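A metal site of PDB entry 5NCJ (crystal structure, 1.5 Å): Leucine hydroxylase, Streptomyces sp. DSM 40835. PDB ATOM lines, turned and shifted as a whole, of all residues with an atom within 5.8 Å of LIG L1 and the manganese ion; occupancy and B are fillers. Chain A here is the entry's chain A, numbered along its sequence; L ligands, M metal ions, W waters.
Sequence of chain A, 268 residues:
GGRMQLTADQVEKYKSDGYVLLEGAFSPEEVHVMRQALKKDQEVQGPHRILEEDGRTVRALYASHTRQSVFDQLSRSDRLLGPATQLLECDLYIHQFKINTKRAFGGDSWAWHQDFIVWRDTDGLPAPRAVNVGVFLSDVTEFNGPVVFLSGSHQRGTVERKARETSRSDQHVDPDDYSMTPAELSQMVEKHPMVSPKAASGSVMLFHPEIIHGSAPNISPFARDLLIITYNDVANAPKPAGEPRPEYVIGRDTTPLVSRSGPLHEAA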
ATOM      1  N   TYR A  62      33.350  -8.412  24.814  1.00  0.00           N
ATOM      2  CA  TYR A  62      31.994  -8.558  24.323  1.00  0.00           C
ATOM      3  C   TYR A  62      31.359  -9.862  24.787  1.00  0.00           C
ATOM      4  O   TYR A  62      32.021 -10.907  24.850  1.00  0.00           O
ATOM      5  CB  TYR A  62      31.941  -8.474  22.790  1.00  0.00           C
ATOM      6  CG  TYR A  62      32.074  -7.046  22.324  1.00  0.00           C
ATOM      7  CD1 TYR A  62      30.965  -6.212  22.249  1.00  0.00           C
ATOM      8  CD2 TYR A  62      33.325  -6.512  22.016  1.00  0.00           C
ATOM      9  CE1 TYR A  62      31.101  -4.892  21.848  1.00  0.00           C
ATOM     10  CE2 TYR A  62      33.451  -5.202  21.621  1.00  0.00           C
ATOM     11  CZ  TYR A  62      32.337  -4.384  21.547  1.00  0.00           C
ATOM     12  OH  TYR A  62      32.436  -3.090  21.151  1.00  0.00           O
ATOM     13  N   GLN A  96      23.610  -5.431  22.508  1.00  0.00           N
ATOM     14  CA  GLN A  96      25.055  -5.456  22.703  1.00  0.00           C
ATOM     15  C   GLN A  96      25.348  -5.543  24.194  1.00  0.00           C
ATOM     16  O   GLN A  96      24.678  -4.908  25.008  1.00  0.00           O
ATOM     17  CB  GLN A  96      25.698  -4.211  22.079  1.00  0.00           C
ATOM     18  CG  GLN A  96      27.212  -4.110  22.216  1.00  0.00           C
ATOM     19  CD  GLN A  96      27.808  -3.124  21.242  1.00  0.00           C
ATOM     20  OE1 GLN A  96      28.202  -2.031  21.624  1.00  0.00           O
ATOM     21  NE2 GLN A  96      27.870  -3.510  19.976  1.00  0.00           N
ATOM     22  N   LYS A  98      28.837  -5.261  26.503  1.00  0.00           N
ATOM     23  CA  LYS A  98      30.263  -5.011  26.506  1.00  0.00           C
ATOM     24  C   LYS A  98      30.709  -4.579  27.883  1.00  0.00           C
ATOM     25  O   LYS A  98      29.954  -4.008  28.661  1.00  0.00           O
ATOM     26  CB  LYS A  98      30.669  -3.961  25.463  1.00  0.00           C
ATOM     27  CG  LYS A  98      29.976  -2.601  25.611  1.00  0.00           C
ATOM     28  CD  LYS A  98      30.529  -1.624  24.545  1.00  0.00           C
ATOM     29  CE  LYS A  98      29.801  -0.318  24.519  1.00  0.00           C
ATOM     30  NZ  LYS A  98      28.392  -0.465  23.986  1.00  0.00           N
ATOM     31  N   ASN A 100      33.921  -2.274  29.043  1.00  0.00           N
ATOM     32  CA  ASN A 100      35.054  -1.435  28.640  1.00  0.00           C
ATOM     33  C   ASN A 100      35.965  -1.293  29.861  1.00  0.00           C
ATOM     34  O   ASN A 100      35.669  -0.538  30.800  1.00  0.00           O
ATOM     35  CB  ASN A 100      34.598  -0.087  28.103  1.00  0.00           C
ATOM     36  CG  ASN A 100      33.931  -0.201  26.730  1.00  0.00           C
ATOM     37  OD1 ASN A 100      34.016  -1.223  26.053  1.00  0.00           O
ATOM     38  ND2 ASN A 100      33.320   0.891  26.295  1.00  0.00           N
ATOM     39  N   TRP A 110      38.104   6.854  24.846  1.00  0.00           N
ATOM     40  CA  TRP A 110      37.043   6.502  23.903  1.00  0.00           C
ATOM     41  C   TRP A 110      36.602   7.790  23.218  1.00  0.00           C
ATOM     42  O   TRP A 110      36.248   8.770  23.885  1.00  0.00           O
ATOM     43  CB  TRP A 110      35.865   5.811  24.605  1.00  0.00           C
ATOM     44  CG  TRP A 110      36.215   4.425  25.131  1.00  0.00           C
ATOM     45  CD1 TRP A 110      36.624   4.095  26.404  1.00  0.00           C
ATOM     46  CD2 TRP A 110      36.219   3.197  24.396  1.00  0.00           C
ATOM     47  NE1 TRP A 110      36.867   2.747  26.498  1.00  0.00           N
ATOM     48  CE2 TRP A 110      36.624   2.178  25.276  1.00  0.00           C
ATOM     49  CE3 TRP A 110      35.886   2.873  23.083  1.00  0.00           C
ATOM     50  CZ2 TRP A 110      36.698   0.842  24.882  1.00  0.00           C
ATOM     51  CZ3 TRP A 110      35.997   1.563  22.685  1.00  0.00           C
ATOM     52  CH2 TRP A 110      36.397   0.553  23.593  1.00  0.00           C
ATOM     53  N   HIS A 113      31.408  10.406  20.365  1.00  0.00           N
ATOM     54  CA  HIS A 113      30.577   9.781  19.340  1.00  0.00           C
ATOM     55  C   HIS A 113      29.133   9.699  19.813  1.00  0.00           C
ATOM     56  O   HIS A 113      28.822   9.881  21.002  1.00  0.00           O
ATOM     57  CB  HIS A 113      31.083   8.381  18.997  1.00  0.00           C
ATOM     58  CG  HIS A 113      30.950   7.404  20.125  1.00  0.00           C
ATOM     59  ND1 HIS A 113      31.745   7.454  21.245  1.00  0.00           N
ATOM     60  CD2 HIS A 113      30.099   6.361  20.319  1.00  0.00           C
ATOM     61  CE1 HIS A 113      31.396   6.478  22.082  1.00  0.00           C
ATOM     62  NE2 HIS A 113      30.400   5.804  21.542  1.00  0.00           N
ATOM     63  N   GLN A 114      28.245   9.390  18.858  1.00  0.00           N
ATOM     64  CA  GLN A 114      26.920   8.835  19.110  1.00  0.00           C
ATOM     65  C   GLN A 114      26.927   7.354  18.764  1.00  0.00           C
ATOM     66  O   GLN A 114      27.564   6.937  17.805  1.00  0.00           O
ATOM     67  CB  GLN A 114      25.854   9.526  18.252  1.00  0.00           C
ATOM     68  CG  GLN A 114      25.740  11.042  18.408  1.00  0.00           C
ATOM     69  CD  GLN A 114      24.733  11.636  17.455  1.00  0.00           C
ATOM     70  OE1 GLN A 114      24.860  11.512  16.219  1.00  0.00           O
ATOM     71  NE2 GLN A 114      23.700  12.267  18.002  1.00  0.00           N
ATOM     72  N   ASP A 115      26.141   6.556  19.522  1.00  0.00           N
ATOM     73  CA  ASP A 115      26.069   5.127  19.254  1.00  0.00           C
ATOM     74  C   ASP A 115      25.199   4.809  18.052  1.00  0.00           C
ATOM     75  O   ASP A 115      25.552   3.953  17.237  1.00  0.00           O
ATOM     76  CB  ASP A 115      25.506   4.364  20.452  1.00  0.00           C
ATOM     77  CG  ASP A 115      26.460   4.271  21.602  1.00  0.00           C
ATOM     78  OD1 ASP A 115      27.679   4.483  21.431  1.00  0.00           O
ATOM     79  OD2 ASP A 115      25.972   3.957  22.696  1.00  0.00           O
ATOM     80  N   VAL A 118      26.253   4.428  14.282  1.00  0.00           N
ATOM     81  CA  VAL A 118      27.107   3.271  14.015  1.00  0.00           C
ATOM     82  C   VAL A 118      26.260   2.039  13.731  1.00  0.00           C
ATOM     83  O   VAL A 118      26.499   1.292  12.778  1.00  0.00           O
ATOM     84  CB  VAL A 118      28.051   3.003  15.192  1.00  0.00           C
ATOM     85  CG1 VAL A 118      28.904   1.761  14.912  1.00  0.00           C
ATOM     86  CG2 VAL A 118      28.917   4.224  15.472  1.00  0.00           C
ATOM     87  N   TRP A 119      25.278   1.796  14.596  1.00  0.00           N
ATOM     88  CA  TRP A 119      24.439   0.608  14.419  1.00  0.00           C
ATOM     89  C   TRP A 119      23.513   0.755  13.221  1.00  0.00           C
ATOM     90  O   TRP A 119      23.247  -0.233  12.533  1.00  0.00           O
ATOM     91  CB  TRP A 119      23.660   0.356  15.708  1.00  0.00           C
ATOM     92  CG  TRP A 119      24.567   0.062  16.890  1.00  0.00           C
ATOM     93  CD1 TRP A 119      25.742  -0.625  16.860  1.00  0.00           C
ATOM     94  CD2 TRP A 119      24.374   0.464  18.264  1.00  0.00           C
ATOM     95  NE1 TRP A 119      26.291  -0.683  18.109  1.00  0.00           N
ATOM     96  CE2 TRP A 119      25.471  -0.043  19.000  1.00  0.00           C
ATOM     97  CE3 TRP A 119      23.378   1.186  18.937  1.00  0.00           C
ATOM     98  CZ2 TRP A 119      25.605   0.162  20.371  1.00  0.00           C
ATOM     99  CZ3 TRP A 119      23.514   1.372  20.322  1.00  0.00           C
ATOM    100  CH2 TRP A 119      24.616   0.862  21.021  1.00  0.00           C
ATOM    101  N   ASP A 123      24.892  -1.935  10.824  1.00  0.00           N
ATOM    102  CA  ASP A 123      24.090  -3.106  11.136  1.00  0.00           C
ATOM    103  C   ASP A 123      22.644  -2.996  10.688  1.00  0.00           C
ATOM    104  O   ASP A 123      21.902  -3.979  10.801  1.00  0.00           O
ATOM    105  CB  ASP A 123      24.143  -3.372  12.646  1.00  0.00           C
ATOM    106  CG  ASP A 123      25.550  -3.443  13.146  1.00  0.00           C
ATOM    107  OD1 ASP A 123      26.275  -4.350  12.671  1.00  0.00           O
ATOM    108  OD2 ASP A 123      25.925  -2.585  13.982  1.00  0.00           O
ATOM    109  N   ASN A 132      21.111   2.372  26.585  1.00  0.00           N
ATOM    110  CA  ASN A 132      22.349   1.866  27.140  1.00  0.00           C
ATOM    111  C   ASN A 132      22.249   1.870  28.659  1.00  0.00           C
ATOM    112  O   ASN A 132      21.856   2.877  29.243  1.00  0.00           O
ATOM    113  CB  ASN A 132      23.531   2.730  26.700  1.00  0.00           C
ATOM    114  CG  ASN A 132      23.734   2.698  25.190  1.00  0.00           C
ATOM    115  OD1 ASN A 132      23.801   1.632  24.579  1.00  0.00           O
ATOM    116  ND2 ASN A 132      23.824   3.879  24.590  1.00  0.00           N
ATOM    117  N   HIS A 172      35.587  -4.907  16.237  1.00  0.00           N
ATOM    118  CA  HIS A 172      34.387  -4.129  16.524  1.00  0.00           C
ATOM    119  C   HIS A 172      34.550  -2.778  15.833  1.00  0.00           C
ATOM    120  O   HIS A 172      35.557  -2.529  15.171  1.00  0.00           O
ATOM    121  CB  HIS A 172      34.139  -3.971  18.031  1.00  0.00           C
ATOM    122  CG  HIS A 172      35.128  -3.104  18.749  1.00  0.00           C
ATOM    123  ND1 HIS A 172      34.814  -2.449  19.918  1.00  0.00           N
ATOM    124  CD2 HIS A 172      36.421  -2.800  18.489  1.00  0.00           C
ATOM    125  CE1 HIS A 172      35.853  -1.762  20.332  1.00  0.00           C
ATOM    126  NE2 HIS A 172      36.842  -1.952  19.487  1.00  0.00           N
ATOM    127  N   VAL A 173      33.558  -1.919  15.970  1.00  0.00           N
ATOM    128  CA  VAL A 173      33.650  -0.557  15.450  1.00  0.00           C
ATOM    129  C   VAL A 173      34.077   0.317  16.614  1.00  0.00           C
ATOM    130  O   VAL A 173      33.288   0.643  17.503  1.00  0.00           O
ATOM    131  CB  VAL A 173      32.324  -0.067  14.839  1.00  0.00           C
ATOM    132  CG1 VAL A 173      32.457   1.385  14.376  1.00  0.00           C
ATOM    133  CG2 VAL A 173      31.934  -0.940  13.669  1.00  0.00           C
ATOM    134  N   ASP A 174      35.359   0.681  16.641  1.00  0.00           N
ATOM    135  CA  ASP A 174      35.810   1.663  17.615  1.00  0.00           C
ATOM    136  C   ASP A 174      35.159   2.999  17.290  1.00  0.00           C
ATOM    137  O   ASP A 174      35.080   3.368  16.114  1.00  0.00           O
ATOM    138  CB  ASP A 174      37.335   1.773  17.562  1.00  0.00           C
ATOM    139  CG  ASP A 174      37.883   2.612  18.697  1.00  0.00           C
ATOM    140  OD1 ASP A 174      37.721   3.842  18.660  1.00  0.00           O
ATOM    141  OD2 ASP A 174      38.459   2.021  19.645  1.00  0.00           O
ATOM    142  N   PRO A 175      34.680   3.744  18.294  1.00  0.00           N
ATOM    143  CA  PRO A 175      34.033   5.029  18.022  1.00  0.00           C
ATOM    144  C   PRO A 175      34.908   6.019  17.257  1.00  0.00           C
ATOM    145  O   PRO A 175      34.349   6.948  16.643  1.00  0.00           O
ATOM    146  CB  PRO A 175      33.681   5.547  19.421  1.00  0.00           C
ATOM    147  CG  PRO A 175      34.473   4.726  20.391  1.00  0.00           C
ATOM    148  CD  PRO A 175      34.678   3.394  19.715  1.00  0.00           C
ATOM    149  N   PHE A 207      21.644   5.673  29.562  1.00  0.00           N
ATOM    150  CA  PHE A 207      21.862   6.772  28.641  1.00  0.00           C
ATOM    151  C   PHE A 207      21.406   6.441  27.228  1.00  0.00           C
ATOM    152  O   PHE A 207      21.360   5.286  26.806  1.00  0.00           O
ATOM    153  CB  PHE A 207      23.324   7.260  28.656  1.00  0.00           C
ATOM    154  CG  PHE A 207      24.380   6.239  28.249  1.00  0.00           C
ATOM    155  CD1 PHE A 207      24.839   5.285  29.149  1.00  0.00           C
ATOM    156  CD2 PHE A 207      24.976   6.299  27.001  1.00  0.00           C
ATOM    157  CE1 PHE A 207      25.854   4.401  28.803  1.00  0.00           C
ATOM    158  CE2 PHE A 207      25.996   5.408  26.651  1.00  0.00           C
ATOM    159  CZ  PHE A 207      26.423   4.469  27.556  1.00  0.00           C
ATOM    160  N   HIS A 213      28.877  11.207  23.698  1.00  0.00           N
ATOM    161  CA  HIS A 213      29.630  10.780  24.865  1.00  0.00           C
ATOM    162  C   HIS A 213      31.020  10.369  24.429  1.00  0.00           C
ATOM    163  O   HIS A 213      31.259  10.053  23.259  1.00  0.00           O
ATOM    164  CB  HIS A 213      28.916   9.661  25.611  1.00  0.00           C
ATOM    165  CG  HIS A 213      28.660   8.431  24.797  1.00  0.00           C
ATOM    166  ND1 HIS A 213      27.715   8.378  23.796  1.00  0.00           N
ATOM    167  CD2 HIS A 213      29.161   7.169  24.902  1.00  0.00           C
ATOM    168  CE1 HIS A 213      27.679   7.163  23.272  1.00  0.00           C
ATOM    169  NE2 HIS A 213      28.552   6.410  23.921  1.00  0.00           N
ATOM    170  N   ARG A 245      27.278  -8.723  11.248  1.00  0.00           N
ATOM    171  CA  ARG A 245      28.426  -8.822  12.118  1.00  0.00           C
ATOM    172  C   ARG A 245      28.217  -9.952  13.115  1.00  0.00           C
ATOM    173  O   ARG A 245      27.109 -10.480  13.259  1.00  0.00           O
ATOM    174  CB  ARG A 245      28.662  -7.492  12.835  1.00  0.00           C
ATOM    175  CG  ARG A 245      29.237  -6.404  11.940  1.00  0.00           C
ATOM    176  CD  ARG A 245      29.976  -5.368  12.770  1.00  0.00           C
ATOM    177  NE  ARG A 245      29.051  -4.530  13.541  1.00  0.00           N
ATOM    178  CZ  ARG A 245      29.387  -3.848  14.631  1.00  0.00           C
ATOM    179  NH1 ARG A 245      30.618  -3.920  15.133  1.00  0.00           N
ATOM    180  NH2 ARG A 245      28.479  -3.087  15.210  1.00  0.00           N
ATOM    181  N   VAL A 249      28.968  -9.117  18.983  1.00  0.00           N
ATOM    182  CA  VAL A 249      28.891  -7.660  18.995  1.00  0.00           C
ATOM    183  C   VAL A 249      27.465  -7.179  18.714  1.00  0.00           C
ATOM    184  O   VAL A 249      27.043  -6.167  19.275  1.00  0.00           O
ATOM    185  CB  VAL A 249      29.935  -7.022  18.038  1.00  0.00           C
ATOM    186  CG1 VAL A 249      29.815  -7.517  16.619  1.00  0.00           C
ATOM    187  CG2 VAL A 249      29.875  -5.507  18.085  1.00  0.00           C
ATOM    188  N   ILE A 250      26.684  -7.922  17.941  1.00  0.00           N
ATOM    189  CA  ILE A 250      25.312  -7.503  17.597  1.00  0.00           C
ATOM    190  C   ILE A 250      24.354  -8.673  17.855  1.00  0.00           C
ATOM    191  O   ILE A 250      24.388  -9.690  17.152  1.00  0.00           O
ATOM    192  CB  ILE A 250      25.199  -7.006  16.142  1.00  0.00           C
ATOM    193  CG1 ILE A 250      26.065  -5.748  15.923  1.00  0.00           C
ATOM    194  CG2 ILE A 250      23.742  -6.706  15.766  1.00  0.00           C
ATOM    195  CD1 ILE A 250      25.656  -4.477  16.714  1.00  0.00           C
HETATM  196  N1  LIG L   1      31.872  -0.711  19.499  1.00  0.00           N
HETATM  197  C1  LIG L   1      30.453  -0.705  19.168  1.00  0.00           C
HETATM  198  C2  LIG L   1      30.134  -1.727  18.084  1.00  0.00           C
HETATM  199  O1  LIG L   1      28.930  -1.930  17.753  1.00  0.00           O
HETATM  200  C3  LIG L   1      30.018   0.685  18.705  1.00  0.00           C
HETATM  201  C4  LIG L   1      30.377   1.781  19.720  1.00  0.00           C
HETATM  202  O2  LIG L   1      29.905   2.608  21.963  1.00  0.00           O
HETATM  203  C5  LIG L   1      29.527   1.652  20.979  1.00  0.00           C
HETATM  204  C6  LIG L   1      30.121   3.128  19.057  1.00  0.00           C
HETATM  205  O3  LIG L   1      31.078  -2.335  17.528  1.00  0.00           O
HETATM  206  C1  LG2 L   2      33.525   4.352  27.633  1.00  0.00           C
HETATM  207  O1  LG2 L   2      33.759   3.196  28.090  1.00  0.00           O
HETATM  208  O2  LG2 L   2      34.060   5.315  28.259  1.00  0.00           O
HETATM  209  C2  LG2 L   2      32.634   4.574  26.436  1.00  0.00           C
HETATM  210  C3  LG2 L   2      31.299   3.879  26.642  1.00  0.00           C
HETATM  211  C4  LG2 L   2      30.423   3.845  25.382  1.00  0.00           C
HETATM  212  O3  LG2 L   2      30.864   4.076  24.236  1.00  0.00           O
HETATM  213  O4  LG2 L   2      29.209   3.577  25.487  1.00  0.00           O
HETATM  214 MN    MN M   1      29.177   4.489  22.901  1.00  0.00          MN
HETATM  215  O   HOH W   1      27.593   2.392  24.234  1.00  0.00           O
HETATM  216  O   HOH W   2      32.553   0.376  21.834  1.00  0.00           O
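The backbone NH of Val 173 is in hydrogen-bond range of an oxygen (O3) of LIG L1 (3.0 Å). A nitrogen (N1) of LIG L1 sits at hydrogen-bond distance from the backbone carbonyl oxygen (O) of Val 173 (2.8 Å). An oxygen (O1) of LIG L1 lies within salt-bridge range of the guanidinium group of Arg 245 (2.8 Å). O1 of LIG L1 sits at hydrogen-bond distance from NE2 of Gln 96, 2.9 Å away. The indole nitrogen of Trp 119 lies within hydrogen-bond range of an oxygen (O1) of LIG L1. N1 of LIG L1 lies within hydrogen-bond range of OH of Tyr 62 (3.0 Å). N1 of LIG L1 is in hydrogen-bond range of ND1 of His 172, at 3.4 Å.
The side-chain amide nitrogen (ND2) of Asn 132 sits at hydrogen-bond distance from the side-chain carboxylate (OD2) of Asp 115 (2.9 Å). The side-chain carboxylate (OD2) of Asp 123 is in salt-bridge range of the guanidinium group (NH2) of Arg 245 (2.9 Å). NE2 of Gln 96 lies within hydrogen-bond range of O of Val 249 (2.9 Å). The side-chain amino group (NZ) of Lys 98 lies within hydrogen-bond range of the side-chain amide oxygen (OE1) of Gln 96, at 2.8 Å. A ring nitrogen (ND1) of His 172 sits at hydrogen-bond distance from the side-chain hydroxyl (OH) of Tyr 62 (2.8 Å).
NZ of Lys 98 touches C5 of LIG L1, at 3.8 Å. Val 118 touches LIG L1. Val 249 touches LIG L1. 11 residues have an atom within 4 Å of LIG L1: Tyr 62, Gln 96, Lys 98, His 113, Asp 115, Val 118, Trp 119, His 172, Val 173, Arg 245 and Val 249. The nearest printed residue that does not touch LIG L1 is Ile 250 (4.3 Å).
Of the 21 residues printed, 3 come within 4 Å of the manganese ion.
The manganese ion is bound by the side-chain carboxylate of Asp 115 (2.1 Å), an oxygen (O3) of LG2 L2 (2.2 Å), an oxygen (O2) of LIG L1 (2.2 Å), a ring nitrogen (NE2) of His 113 (2.3 Å) and a ring nitrogen (NE2) of His 213 (2.3 Å). The manganese ion has five donor atoms within binding distance. Slightly farther from the manganese ion lies O4 of LG2 L2 (2.7 Å). Slightly farther from the manganese ion lies water W1 (2.9 Å).
Water W1 lies within hydrogen-bond range of OD2 of Asp 115 (2.7 Å) and NZ of Lys 98 (3.0 Å).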
